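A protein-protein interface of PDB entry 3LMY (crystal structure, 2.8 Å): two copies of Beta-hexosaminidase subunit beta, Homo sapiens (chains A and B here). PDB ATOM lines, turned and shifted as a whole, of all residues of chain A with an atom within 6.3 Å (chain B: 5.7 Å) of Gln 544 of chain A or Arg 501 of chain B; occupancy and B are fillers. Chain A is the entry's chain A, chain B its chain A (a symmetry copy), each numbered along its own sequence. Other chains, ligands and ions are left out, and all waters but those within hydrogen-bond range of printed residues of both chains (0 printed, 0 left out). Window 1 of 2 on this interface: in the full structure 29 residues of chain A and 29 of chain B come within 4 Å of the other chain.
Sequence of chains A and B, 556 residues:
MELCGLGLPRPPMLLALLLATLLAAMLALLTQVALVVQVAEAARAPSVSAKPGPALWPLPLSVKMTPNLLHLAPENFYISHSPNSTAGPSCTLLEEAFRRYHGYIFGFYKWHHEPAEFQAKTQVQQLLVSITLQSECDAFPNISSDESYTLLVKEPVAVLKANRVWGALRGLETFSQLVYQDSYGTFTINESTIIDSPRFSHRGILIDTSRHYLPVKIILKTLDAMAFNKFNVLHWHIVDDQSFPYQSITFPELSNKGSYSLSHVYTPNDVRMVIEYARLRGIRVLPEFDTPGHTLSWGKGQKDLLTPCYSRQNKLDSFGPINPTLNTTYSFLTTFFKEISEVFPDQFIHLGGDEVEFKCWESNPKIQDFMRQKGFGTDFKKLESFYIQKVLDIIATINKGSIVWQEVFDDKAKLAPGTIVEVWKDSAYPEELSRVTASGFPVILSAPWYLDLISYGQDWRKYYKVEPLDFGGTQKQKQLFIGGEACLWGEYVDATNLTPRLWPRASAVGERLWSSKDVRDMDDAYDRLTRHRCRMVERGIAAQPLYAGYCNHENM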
ATOM      1  N   SER A 455     -24.192  -5.718 -33.988  1.00  0.00           N
ATOM      2  CA  SER A 455     -24.152  -4.406 -33.336  1.00  0.00           C
ATOM      3  C   SER A 455     -24.299  -4.584 -31.838  1.00  0.00           C
ATOM      4  O   SER A 455     -24.642  -5.674 -31.386  1.00  0.00           O
ATOM      5  CB  SER A 455     -25.259  -3.463 -33.863  1.00  0.00           C
ATOM      6  OG  SER A 455     -26.562  -3.861 -33.442  1.00  0.00           O
ATOM      7  N   ASP A 459     -29.813  -6.925 -29.748  1.00  0.00           N
ATOM      8  CA  ASP A 459     -30.421  -6.795 -31.107  1.00  0.00           C
ATOM      9  C   ASP A 459     -31.458  -7.884 -31.481  1.00  0.00           C
ATOM     10  O   ASP A 459     -32.185  -7.739 -32.508  1.00  0.00           O
ATOM     11  CB  ASP A 459     -29.374  -6.581 -32.235  1.00  0.00           C
ATOM     12  CG  ASP A 459     -28.410  -7.761 -32.399  1.00  0.00           C
ATOM     13  OD1 ASP A 459     -28.509  -8.728 -31.612  1.00  0.00           O
ATOM     14  OD2 ASP A 459     -27.539  -7.732 -33.310  1.00  0.00           O
ATOM     15  N   THR A 499     -20.932 -19.806 -33.974  1.00  0.00           N
ATOM     16  CA  THR A 499     -21.999 -20.262 -33.091  1.00  0.00           C
ATOM     17  C   THR A 499     -22.486 -19.173 -32.152  1.00  0.00           C
ATOM     18  O   THR A 499     -23.711 -18.884 -32.082  1.00  0.00           O
ATOM     19  CB  THR A 499     -21.531 -21.444 -32.303  1.00  0.00           C
ATOM     20  OG1 THR A 499     -21.420 -22.521 -33.212  1.00  0.00           O
ATOM     21  CG2 THR A 499     -22.502 -21.822 -31.184  1.00  0.00           C
ATOM     22  N   PRO A 500     -21.547 -18.580 -31.398  1.00  0.00           N
ATOM     23  CA  PRO A 500     -22.037 -17.515 -30.523  1.00  0.00           C
ATOM     24  C   PRO A 500     -22.599 -16.345 -31.346  1.00  0.00           C
ATOM     25  O   PRO A 500     -23.362 -15.520 -30.836  1.00  0.00           O
ATOM     26  CB  PRO A 500     -20.803 -17.122 -29.715  1.00  0.00           C
ATOM     27  CG  PRO A 500     -19.605 -17.889 -30.419  1.00  0.00           C
ATOM     28  CD  PRO A 500     -20.195 -19.051 -31.039  1.00  0.00           C
ATOM     29  N   ARG A 501     -22.262 -16.295 -32.628  1.00  0.00           N
ATOM     30  CA  ARG A 501     -22.755 -15.169 -33.395  1.00  0.00           C
ATOM     31  C   ARG A 501     -24.173 -15.443 -33.795  1.00  0.00           C
ATOM     32  O   ARG A 501     -24.983 -14.516 -33.728  1.00  0.00           O
ATOM     33  CB  ARG A 501     -21.904 -14.837 -34.622  1.00  0.00           C
ATOM     34  CG  ARG A 501     -22.433 -13.623 -35.314  1.00  0.00           C
ATOM     35  CD  ARG A 501     -21.451 -12.931 -36.160  1.00  0.00           C
ATOM     36  NE  ARG A 501     -20.423 -12.222 -35.403  1.00  0.00           N
ATOM     37  CZ  ARG A 501     -19.314 -11.781 -35.990  1.00  0.00           C
ATOM     38  NH1 ARG A 501     -19.145 -11.987 -37.286  1.00  0.00           N
ATOM     39  NH2 ARG A 501     -18.365 -11.165 -35.331  1.00  0.00           N
ATOM     40  N   LEU A 502     -24.447 -16.702 -34.201  1.00  0.00           N
ATOM     41  CA  LEU A 502     -25.750 -17.193 -34.648  1.00  0.00           C
ATOM     42  C   LEU A 502     -26.746 -17.301 -33.527  1.00  0.00           C
ATOM     43  O   LEU A 502     -27.893 -16.960 -33.712  1.00  0.00           O
ATOM     44  CB  LEU A 502     -25.612 -18.595 -35.240  1.00  0.00           C
ATOM     45  CG  LEU A 502     -26.027 -18.843 -36.691  1.00  0.00           C
ATOM     46  CD1 LEU A 502     -26.030 -20.326 -36.970  1.00  0.00           C
ATOM     47  CD2 LEU A 502     -27.362 -18.203 -37.073  1.00  0.00           C
ATOM     48  N   TRP A 503     -26.314 -17.766 -32.362  1.00  0.00           N
ATOM     49  CA  TRP A 503     -27.263 -18.188 -31.354  1.00  0.00           C
ATOM     50  C   TRP A 503     -27.046 -17.438 -30.036  1.00  0.00           C
ATOM     51  O   TRP A 503     -25.870 -17.265 -29.592  1.00  0.00           O
ATOM     52  CB  TRP A 503     -27.176 -19.693 -31.115  1.00  0.00           C
ATOM     53  CG  TRP A 503     -27.252 -20.571 -32.330  1.00  0.00           C
ATOM     54  CD1 TRP A 503     -26.227 -21.303 -32.890  1.00  0.00           C
ATOM     55  CD2 TRP A 503     -28.424 -20.858 -33.118  1.00  0.00           C
ATOM     56  NE1 TRP A 503     -26.683 -22.011 -33.993  1.00  0.00           N
ATOM     57  CE2 TRP A 503     -28.021 -21.759 -34.158  1.00  0.00           C
ATOM     58  CE3 TRP A 503     -29.781 -20.473 -33.032  1.00  0.00           C
ATOM     59  CZ2 TRP A 503     -28.929 -22.269 -35.106  1.00  0.00           C
ATOM     60  CZ3 TRP A 503     -30.680 -20.960 -33.988  1.00  0.00           C
ATOM     61  CH2 TRP A 503     -30.251 -21.846 -35.009  1.00  0.00           C
ATOM     62  N   PRO A 504     -28.156 -16.974 -29.393  1.00  0.00           N
ATOM     63  CA  PRO A 504     -29.572 -17.137 -29.700  1.00  0.00           C
ATOM     64  C   PRO A 504     -30.198 -16.160 -30.706  1.00  0.00           C
ATOM     65  O   PRO A 504     -31.431 -16.159 -30.890  1.00  0.00           O
ATOM     66  CB  PRO A 504     -30.239 -16.938 -28.327  1.00  0.00           C
ATOM     67  CG  PRO A 504     -29.373 -16.044 -27.601  1.00  0.00           C
ATOM     68  CD  PRO A 504     -27.982 -16.095 -28.221  1.00  0.00           C
ATOM     69  N   ARG A 505     -29.383 -15.335 -31.354  1.00  0.00           N
ATOM     70  CA  ARG A 505     -29.949 -14.268 -32.204  1.00  0.00           C
ATOM     71  C   ARG A 505     -30.945 -14.815 -33.270  1.00  0.00           C
ATOM     72  O   ARG A 505     -32.056 -14.250 -33.465  1.00  0.00           O
ATOM     73  CB  ARG A 505     -28.834 -13.399 -32.798  1.00  0.00           C
ATOM     74  CG  ARG A 505     -28.293 -12.366 -31.791  1.00  0.00           C
ATOM     75  CD  ARG A 505     -27.596 -11.178 -32.471  1.00  0.00           C
ATOM     76  NE  ARG A 505     -26.648 -11.707 -33.417  1.00  0.00           N
ATOM     77  CZ  ARG A 505     -26.333 -11.155 -34.576  1.00  0.00           C
ATOM     78  NH1 ARG A 505     -26.868  -9.993 -34.971  1.00  0.00           N
ATOM     79  NH2 ARG A 505     -25.472 -11.802 -35.344  1.00  0.00           N
ATOM     80  N   ARG A 533     -31.700 -20.381 -24.098  1.00  0.00           N
ATOM     81  CA  ARG A 533     -30.290 -20.233 -24.373  1.00  0.00           C
ATOM     82  C   ARG A 533     -29.448 -21.081 -23.429  1.00  0.00           C
ATOM     83  O   ARG A 533     -28.539 -21.749 -23.906  1.00  0.00           O
ATOM     84  CB  ARG A 533     -29.894 -18.755 -24.348  1.00  0.00           C
ATOM     85  CG  ARG A 533     -28.436 -18.480 -24.585  1.00  0.00           C
ATOM     86  CD  ARG A 533     -27.734 -18.141 -23.293  1.00  0.00           C
ATOM     87  NE  ARG A 533     -26.300 -18.228 -23.505  1.00  0.00           N
ATOM     88  CZ  ARG A 533     -25.389 -17.890 -22.602  1.00  0.00           C
ATOM     89  NH1 ARG A 533     -25.788 -17.438 -21.445  1.00  0.00           N
ATOM     90  NH2 ARG A 533     -24.083 -17.979 -22.866  1.00  0.00           N
ATOM     91  N   VAL A 537     -26.756 -24.116 -24.455  1.00  0.00           N
ATOM     92  CA  VAL A 537     -25.422 -24.218 -23.878  1.00  0.00           C
ATOM     93  C   VAL A 537     -25.246 -25.597 -23.240  1.00  0.00           C
ATOM     94  O   VAL A 537     -24.208 -26.247 -23.392  1.00  0.00           O
ATOM     95  CB  VAL A 537     -25.176 -23.090 -22.857  1.00  0.00           C
ATOM     96  CG1 VAL A 537     -23.926 -23.289 -22.165  1.00  0.00           C
ATOM     97  CG2 VAL A 537     -25.143 -21.751 -23.553  1.00  0.00           C
ATOM     98  N   ILE A 541     -24.220 -26.254 -27.517  1.00  0.00           N
ATOM     99  CA  ILE A 541     -24.194 -25.163 -28.456  1.00  0.00           C
ATOM    100  C   ILE A 541     -23.664 -23.916 -27.726  1.00  0.00           C
ATOM    101  O   ILE A 541     -24.290 -23.426 -26.768  1.00  0.00           O
ATOM    102  CB  ILE A 541     -25.613 -24.888 -28.923  1.00  0.00           C
ATOM    103  CG1 ILE A 541     -26.231 -26.185 -29.458  1.00  0.00           C
ATOM    104  CG2 ILE A 541     -25.661 -23.685 -29.902  1.00  0.00           C
ATOM    105  CD1 ILE A 541     -25.503 -26.789 -30.663  1.00  0.00           C
ATOM    106  N   ALA A 542     -22.533 -23.370 -28.154  1.00  0.00           N
ATOM    107  CA  ALA A 542     -21.954 -22.260 -27.408  1.00  0.00           C
ATOM    108  C   ALA A 542     -22.711 -20.946 -27.644  1.00  0.00           C
ATOM    109  O   ALA A 542     -22.111 -19.945 -28.030  1.00  0.00           O
ATOM    110  CB  ALA A 542     -20.506 -22.109 -27.753  1.00  0.00           C
ATOM    111  N   ALA A 543     -24.014 -20.921 -27.418  1.00  0.00           N
ATOM    112  CA  ALA A 543     -24.757 -19.733 -27.746  1.00  0.00           C
ATOM    113  C   ALA A 543     -24.477 -18.607 -26.710  1.00  0.00           C
ATOM    114  O   ALA A 543     -24.288 -18.886 -25.497  1.00  0.00           O
ATOM    115  CB  ALA A 543     -26.227 -20.054 -27.872  1.00  0.00           C
ATOM    116  N   GLN A 544     -24.435 -17.353 -27.202  1.00  0.00           N
ATOM    117  CA  GLN A 544     -23.949 -16.203 -26.422  1.00  0.00           C
ATOM    118  C   GLN A 544     -25.009 -15.642 -25.495  1.00  0.00           C
ATOM    119  O   GLN A 544     -26.171 -15.949 -25.655  1.00  0.00           O
ATOM    120  CB  GLN A 544     -23.509 -15.124 -27.374  1.00  0.00           C
ATOM    121  CG  GLN A 544     -24.608 -14.467 -28.160  1.00  0.00           C
ATOM    122  CD  GLN A 544     -24.040 -13.403 -29.044  1.00  0.00           C
ATOM    123  OE1 GLN A 544     -22.863 -13.118 -28.970  1.00  0.00           O
ATOM    124  NE2 GLN A 544     -24.844 -12.828 -29.889  1.00  0.00           N
ATOM    125  N   PRO A 545     -24.633 -14.805 -24.527  1.00  0.00           N
ATOM    126  CA  PRO A 545     -25.678 -14.316 -23.623  1.00  0.00           C
ATOM    127  C   PRO A 545     -26.676 -13.321 -24.276  1.00  0.00           C
ATOM    128  O   PRO A 545     -26.420 -12.812 -25.373  1.00  0.00           O
ATOM    129  CB  PRO A 545     -24.883 -13.592 -22.541  1.00  0.00           C
ATOM    130  CG  PRO A 545     -23.551 -14.093 -22.632  1.00  0.00           C
ATOM    131  CD  PRO A 545     -23.291 -14.461 -24.046  1.00  0.00           C
ATOM    132  N   LEU A 546     -27.808 -13.061 -23.611  1.00  0.00           N
ATOM    133  CA  LEU A 546     -28.757 -12.008 -24.011  1.00  0.00           C
ATOM    134  C   LEU A 546     -28.428 -10.719 -23.242  1.00  0.00           C
ATOM    135  O   LEU A 546     -28.540  -9.593 -23.782  1.00  0.00           O
ATOM    136  CB  LEU A 546     -30.200 -12.432 -23.694  1.00  0.00           C
ATOM    137  CG  LEU A 546     -30.960 -13.427 -24.564  1.00  0.00           C
ATOM    138  CD1 LEU A 546     -32.397 -13.533 -24.144  1.00  0.00           C
ATOM    139  CD2 LEU A 546     -30.951 -12.936 -25.976  1.00  0.00           C
ATOM    140  N   LEU B 451     -14.266  -2.397 -26.759  1.00  0.00           N
ATOM    141  CA  LEU B 451     -14.390  -3.564 -27.602  1.00  0.00           C
ATOM    142  C   LEU B 451     -15.710  -4.282 -27.434  1.00  0.00           C
ATOM    143  O   LEU B 451     -16.089  -5.025 -28.312  1.00  0.00           O
ATOM    144  CB  LEU B 451     -13.213  -4.530 -27.433  1.00  0.00           C
ATOM    145  CG  LEU B 451     -11.780  -4.122 -27.845  1.00  0.00           C
ATOM    146  CD1 LEU B 451     -11.086  -5.291 -28.502  1.00  0.00           C
ATOM    147  CD2 LEU B 451     -11.684  -2.896 -28.754  1.00  0.00           C
ATOM    148  N   ASP B 452     -16.433  -4.064 -26.342  1.00  0.00           N
ATOM    149  CA  ASP B 452     -17.794  -4.597 -26.242  1.00  0.00           C
ATOM    150  C   ASP B 452     -18.719  -3.897 -27.252  1.00  0.00           C
ATOM    151  O   ASP B 452     -19.766  -4.435 -27.614  1.00  0.00           O
ATOM    152  CB  ASP B 452     -18.347  -4.443 -24.820  1.00  0.00           C
ATOM    153  CG  ASP B 452     -18.248  -3.020 -24.323  1.00  0.00           C
ATOM    154  OD1 ASP B 452     -17.068  -2.537 -24.271  1.00  0.00           O
ATOM    155  OD2 ASP B 452     -19.333  -2.395 -24.018  1.00  0.00           O
ATOM    156  N   ILE B 454     -19.320  -3.664 -30.339  1.00  0.00           N
ATOM    157  CA  ILE B 454     -19.054  -4.350 -31.608  1.00  0.00           C
ATOM    158  C   ILE B 454     -19.850  -3.723 -32.760  1.00  0.00           C
ATOM    159  O   ILE B 454     -20.873  -3.047 -32.533  1.00  0.00           O
ATOM    160  CB  ILE B 454     -19.445  -5.818 -31.494  1.00  0.00           C
ATOM    161  CG1 ILE B 454     -20.927  -5.928 -31.099  1.00  0.00           C
ATOM    162  CG2 ILE B 454     -18.565  -6.523 -30.481  1.00  0.00           C
ATOM    163  CD1 ILE B 454     -21.582  -7.209 -31.486  1.00  0.00           C
ATOM    164  N   LEU B 488     -13.304  -4.764 -22.563  1.00  0.00           N
ATOM    165  CA  LEU B 488     -14.382  -5.640 -22.925  1.00  0.00           C
ATOM    166  C   LEU B 488     -15.347  -5.770 -21.757  1.00  0.00           C
ATOM    167  O   LEU B 488     -15.137  -6.596 -20.871  1.00  0.00           O
ATOM    168  CB  LEU B 488     -13.806  -6.964 -23.346  1.00  0.00           C
ATOM    169  CG  LEU B 488     -14.866  -7.858 -23.955  1.00  0.00           C
ATOM    170  CD1 LEU B 488     -15.688  -7.143 -25.045  1.00  0.00           C
ATOM    171  CD2 LEU B 488     -14.227  -9.195 -24.447  1.00  0.00           C
ATOM    172  N   TYR B 492     -22.685  -8.274 -22.376  1.00  0.00           N
ATOM    173  CA  TYR B 492     -23.024  -9.189 -23.455  1.00  0.00           C
ATOM    174  C   TYR B 492     -21.967 -10.268 -23.622  1.00  0.00           C
ATOM    175  O   TYR B 492     -21.922 -10.931 -24.636  1.00  0.00           O
ATOM    176  CB  TYR B 492     -23.291  -8.400 -24.743  1.00  0.00           C
ATOM    177  CG  TYR B 492     -24.340  -7.350 -24.476  1.00  0.00           C
ATOM    178  CD1 TYR B 492     -25.666  -7.723 -24.247  1.00  0.00           C
ATOM    179  CD2 TYR B 492     -24.009  -5.992 -24.348  1.00  0.00           C
ATOM    180  CE1 TYR B 492     -26.639  -6.795 -23.943  1.00  0.00           C
ATOM    181  CE2 TYR B 492     -24.996  -5.039 -24.048  1.00  0.00           C
ATOM    182  CZ  TYR B 492     -26.304  -5.459 -23.848  1.00  0.00           C
ATOM    183  OH  TYR B 492     -27.298  -4.578 -23.531  1.00  0.00           O
ATOM    184  N   VAL B 493     -21.128 -10.477 -22.611  1.00  0.00           N
ATOM    185  CA  VAL B 493     -19.957 -11.329 -22.817  1.00  0.00           C
ATOM    186  C   VAL B 493     -19.829 -12.409 -21.784  1.00  0.00           C
ATOM    187  O   VAL B 493     -20.001 -12.146 -20.602  1.00  0.00           O
ATOM    188  CB  VAL B 493     -18.633 -10.520 -22.786  1.00  0.00           C
ATOM    189  CG1 VAL B 493     -17.470 -11.453 -22.982  1.00  0.00           C
ATOM    190  CG2 VAL B 493     -18.618  -9.457 -23.893  1.00  0.00           C
ATOM    191  N   ASP B 494     -19.497 -13.614 -22.213  1.00  0.00           N
ATOM    192  CA  ASP B 494     -19.040 -14.613 -21.260  1.00  0.00           C
ATOM    193  C   ASP B 494     -18.172 -15.678 -21.935  1.00  0.00           C
ATOM    194  O   ASP B 494     -17.764 -15.506 -23.077  1.00  0.00           O
ATOM    195  CB  ASP B 494     -20.203 -15.223 -20.444  1.00  0.00           C
ATOM    196  CG  ASP B 494     -21.145 -16.112 -21.267  1.00  0.00           C
ATOM    197  OD1 ASP B 494     -20.841 -16.494 -22.425  1.00  0.00           O
ATOM    198  OD2 ASP B 494     -22.232 -16.443 -20.732  1.00  0.00           O
ATOM    199  N   THR B 496     -18.718 -18.228 -23.558  1.00  0.00           N
ATOM    200  CA  THR B 496     -19.149 -18.625 -24.898  1.00  0.00           C
ATOM    201  C   THR B 496     -18.707 -17.652 -25.995  1.00  0.00           C
ATOM    202  O   THR B 496     -18.599 -18.052 -27.154  1.00  0.00           O
ATOM    203  CB  THR B 496     -20.678 -18.782 -25.035  1.00  0.00           C
ATOM    204  OG1 THR B 496     -21.323 -17.526 -24.730  1.00  0.00           O
ATOM    205  CG2 THR B 496     -21.216 -19.955 -24.173  1.00  0.00           C
ATOM    206  N   ASN B 497     -18.462 -16.381 -25.674  1.00  0.00           N
ATOM    207  CA  ASN B 497     -18.131 -15.451 -26.773  1.00  0.00           C
ATOM    208  C   ASN B 497     -16.932 -14.480 -26.615  1.00  0.00           C
ATOM    209  O   ASN B 497     -16.617 -13.715 -27.551  1.00  0.00           O
ATOM    210  CB  ASN B 497     -19.389 -14.708 -27.224  1.00  0.00           C
ATOM    211  CG  ASN B 497     -19.830 -13.645 -26.256  1.00  0.00           C
ATOM    212  OD1 ASN B 497     -19.391 -13.572 -25.103  1.00  0.00           O
ATOM    213  ND2 ASN B 497     -20.702 -12.800 -26.730  1.00  0.00           N
ATOM    214  N   LEU B 498     -16.261 -14.574 -25.465  1.00  0.00           N
ATOM    215  CA  LEU B 498     -15.291 -13.593 -24.993  1.00  0.00           C
ATOM    216  C   LEU B 498     -14.036 -13.524 -25.865  1.00  0.00           C
ATOM    217  O   LEU B 498     -13.541 -12.414 -26.156  1.00  0.00           O
ATOM    218  CB  LEU B 498     -14.882 -13.901 -23.545  1.00  0.00           C
ATOM    219  CG  LEU B 498     -13.742 -13.051 -22.988  1.00  0.00           C
ATOM    220  CD1 LEU B 498     -13.830 -12.975 -21.481  1.00  0.00           C
ATOM    221  CD2 LEU B 498     -12.412 -13.574 -23.396  1.00  0.00           C
ATOM    222  N   THR B 499     -13.527 -14.691 -26.277  1.00  0.00           N
ATOM    223  CA  THR B 499     -12.258 -14.785 -26.988  1.00  0.00           C
ATOM    224  C   THR B 499     -12.353 -14.291 -28.421  1.00  0.00           C
ATOM    225  O   THR B 499     -11.555 -13.415 -28.853  1.00  0.00           O
ATOM    226  CB  THR B 499     -11.773 -16.201 -26.969  1.00  0.00           C
ATOM    227  OG1 THR B 499     -11.386 -16.478 -25.637  1.00  0.00           O
ATOM    228  CG2 THR B 499     -10.581 -16.423 -27.900  1.00  0.00           C
ATOM    229  N   PRO B 500     -13.300 -14.862 -29.182  1.00  0.00           N
ATOM    230  CA  PRO B 500     -13.390 -14.347 -30.548  1.00  0.00           C
ATOM    231  C   PRO B 500     -13.801 -12.866 -30.550  1.00  0.00           C
ATOM    232  O   PRO B 500     -13.602 -12.155 -31.538  1.00  0.00           O
ATOM    233  CB  PRO B 500     -14.438 -15.247 -31.199  1.00  0.00           C
ATOM    234  CG  PRO B 500     -15.047 -16.084 -29.995  1.00  0.00           C
ATOM    235  CD  PRO B 500     -14.009 -16.143 -28.996  1.00  0.00           C
ATOM    236  N   ARG B 501     -14.332 -12.389 -29.432  1.00  0.00           N
ATOM    237  CA  ARG B 501     -14.761 -11.004 -29.448  1.00  0.00           C
ATOM    238  C   ARG B 501     -13.564 -10.128 -29.235  1.00  0.00           C
ATOM    239  O   ARG B 501     -13.471  -9.100 -29.910  1.00  0.00           O
ATOM    240  CB  ARG B 501     -15.851 -10.684 -28.423  1.00  0.00           C
ATOM    241  CG  ARG B 501     -16.290  -9.263 -28.551  1.00  0.00           C
ATOM    242  CD  ARG B 501     -17.626  -8.988 -28.006  1.00  0.00           C
ATOM    243  NE  ARG B 501     -18.712  -9.542 -28.812  1.00  0.00           N
ATOM    244  CZ  ARG B 501     -19.950  -9.632 -28.334  1.00  0.00           C
ATOM    245  NH1 ARG B 501     -20.199  -9.205 -27.106  1.00  0.00           N
ATOM    246  NH2 ARG B 501     -20.936 -10.146 -29.025  1.00  0.00           N
ATOM    247  N   LEU B 502     -12.675 -10.544 -28.307  1.00  0.00           N
ATOM    248  CA  LEU B 502     -11.447  -9.848 -27.924  1.00  0.00           C
ATOM    249  C   LEU B 502     -10.397  -9.888 -28.999  1.00  0.00           C
ATOM    250  O   LEU B 502      -9.738  -8.898 -29.227  1.00  0.00           O
ATOM    251  CB  LEU B 502     -10.829 -10.505 -26.691  1.00  0.00           C
ATOM    252  CG  LEU B 502     -10.627  -9.679 -25.420  1.00  0.00           C
ATOM    253  CD1 LEU B 502      -9.792 -10.461 -24.436  1.00  0.00           C
ATOM    254  CD2 LEU B 502     -10.036  -8.291 -25.670  1.00  0.00           C
ATOM    255  N   TRP B 503     -10.241 -11.024 -29.665  1.00  0.00           N
ATOM    256  CA  TRP B 503      -9.060 -11.232 -30.478  1.00  0.00           C
ATOM    257  C   TRP B 503      -9.433 -11.559 -31.927  1.00  0.00           C
ATOM    258  O   TRP B 503     -10.372 -12.376 -32.170  1.00  0.00           O
ATOM    259  CB  TRP B 503      -8.187 -12.343 -29.902  1.00  0.00           C
ATOM    260  CG  TRP B 503      -7.830 -12.231 -28.449  1.00  0.00           C
ATOM    261  CD1 TRP B 503      -8.298 -13.016 -27.416  1.00  0.00           C
ATOM    262  CD2 TRP B 503      -6.889 -11.313 -27.857  1.00  0.00           C
ATOM    263  NE1 TRP B 503      -7.724 -12.628 -26.214  1.00  0.00           N
ATOM    264  CE2 TRP B 503      -6.860 -11.590 -26.450  1.00  0.00           C
ATOM    265  CE3 TRP B 503      -6.043 -10.308 -28.376  1.00  0.00           C
ATOM    266  CZ2 TRP B 503      -6.023 -10.887 -25.562  1.00  0.00           C
ATOM    267  CZ3 TRP B 503      -5.228  -9.591 -27.491  1.00  0.00           C
ATOM    268  CH2 TRP B 503      -5.224  -9.884 -26.103  1.00  0.00           C
ATOM    269  N   ARG B 505      -9.106  -8.189 -32.313  1.00  0.00           N
ATOM    270  CA  ARG B 505      -9.457  -6.756 -32.241  1.00  0.00           C
ATOM    271  C   ARG B 505      -8.551  -5.964 -31.251  1.00  0.00           C
ATOM    272  O   ARG B 505      -8.057  -4.850 -31.578  1.00  0.00           O
ATOM    273  CB  ARG B 505     -10.957  -6.578 -31.973  1.00  0.00           C
ATOM    274  CG  ARG B 505     -11.808  -6.765 -33.243  1.00  0.00           C
ATOM    275  CD  ARG B 505     -13.188  -6.096 -33.141  1.00  0.00           C
ATOM    276  NE  ARG B 505     -13.788  -6.512 -31.900  1.00  0.00           N
ATOM    277  CZ  ARG B 505     -14.578  -5.771 -31.144  1.00  0.00           C
ATOM    278  NH1 ARG B 505     -14.926  -4.527 -31.498  1.00  0.00           N
ATOM    279  NH2 ARG B 505     -15.008  -6.299 -30.011  1.00  0.00           N
ATOM    280  N   GLN B 544     -10.996 -14.496 -33.874  1.00  0.00           N
ATOM    281  CA  GLN B 544     -11.917 -14.461 -35.022  1.00  0.00           C
ATOM    282  C   GLN B 544     -11.252 -13.948 -36.283  1.00  0.00           C
ATOM    283  O   GLN B 544     -10.191 -13.366 -36.209  1.00  0.00           O
ATOM    284  CB  GLN B 544     -13.081 -13.570 -34.683  1.00  0.00           C
ATOM    285  CG  GLN B 544     -12.760 -12.108 -34.557  1.00  0.00           C
ATOM    286  CD  GLN B 544     -14.002 -11.336 -34.245  1.00  0.00           C
ATOM    287  OE1 GLN B 544     -15.078 -11.897 -34.232  1.00  0.00           O
ATOM    288  NE2 GLN B 544     -13.874 -10.071 -33.972  1.00  0.00           N
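Arg 501 of chain A touches Gln 544 of chain B, and with the chains exchanged Gln 544 of chain A touches Arg 501 of chain B.
Of the 15 pairs that touch across the chains among the printed residues, 2 have their exchanged pair printed and touching as well.
Of chain B, only Thr 496 (3.4 Å), Asn 497 (3.1 Å) and Arg 501 (3.5 Å) come within 4 Å of Gln 544 of chain A.
Of chain A, only Gln 544 comes within 4 Å of Arg 501 of chain B.
Of the printed residues of chain A, Thr 496 of chain B touches Pro 500, Arg 533, Ala 542, Ala 543, Gln 544 and Pro 545.
Printed residues of chain A within 4 Å of Gln 544 of chain B: Arg 501.
Val 537 of chain A touches none of the printed residues of chain B.
Leu 498 of chain B touches none of the printed residues of chain A.
The nearest residue of chain B that does not touch Gln 544 of chain A is Tyr 492 of chain B (4.9 Å).
The nearest printed residue of chain B that does not touch Pro 500 of chain A is Pro 500 of chain B (4.9 Å).
Of the 17 printed residues of chain B, 7 touch a printed residue of chain A.
Along chain B the printed residues that touch a printed residue of chain A span positions 454 to 544.
Of the 17 printed residues of chain A, 9 touch a printed residue of chain B.
Hydrophobic or aromatic side chains of chain A that line the printed part of chain B: Pro 500 and Pro 545.
The guanidinium group (NH2) of Arg 533 of chain A lies within salt-bridge range of the side-chain carboxylate (OD2) of Asp 494 of chain B, at 3.2 Å.
NH2 of Arg 533 of chain A lies within hydrogen-bond range of OG1 of Thr 496 of chain B, 3.4 Å away.
The backbone carbonyl oxygen of Ala 543 of chain A is in hydrogen-bond range of the side-chain hydroxyl of Thr 496 of chain B.
The side-chain amide oxygen of Gln 544 of chain A sits at hydrogen-bond distance from the side-chain amide nitrogen of Asn 497 of chain B (3.1 Å).
Among the printed residues, merely in contact across the chains: Ser 455 of chain A with Ile 454 of chain B (3.4 Å), Pro 500 of chain A with Thr 496 of chain B (3.4 Å), Pro 500 of chain A with Asn 497 of chain B (3.7 Å), Arg 501 of chain A with Gln 544 of chain B (3.5 Å), Ala 542 of chain A with Thr 496 of chain B (3.5 Å), Gln 544 of chain A with Thr 496 of chain B (3.4 Å), Gln 544 of chain A with Arg 501 of chain B (3.5 Å), Pro 545 of chain A with Tyr 492 of chain B (3.8 Å), Pro 545 of chain A with Asp 494 of chain B (3.3 Å), Pro 545 of chain A with Thr 496 of chain B (3.7 Å) and Leu 546 of chain A with Tyr 492 of chain B (3.4 Å).
OE1 of Gln 544 of chain A lies close to O of Pro 500 of chain A (3.1 Å).
O of Tyr 492 of chain B sits at hydrogen-bond distance from ND2 of Asn 497 of chain B (3.1 Å).
OD1 of Asn 497 of chain B lies within hydrogen-bond range of N of Asp 494 of chain B (2.9 Å).
O of Pro 500 of chain B sits close to OE1 of Gln 544 of chain B (3.1 Å).
The backbone carbonyl oxygen of Arg 501 of chain B is in hydrogen-bond range of the guanidinium group of Arg 505 of chain B (3.2 Å).
The backbone NH (N) of Gln 544 of chain B lies within hydrogen-bond range of the backbone carbonyl oxygen (O) of Trp 503 of chain B, 2.8 Å away.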
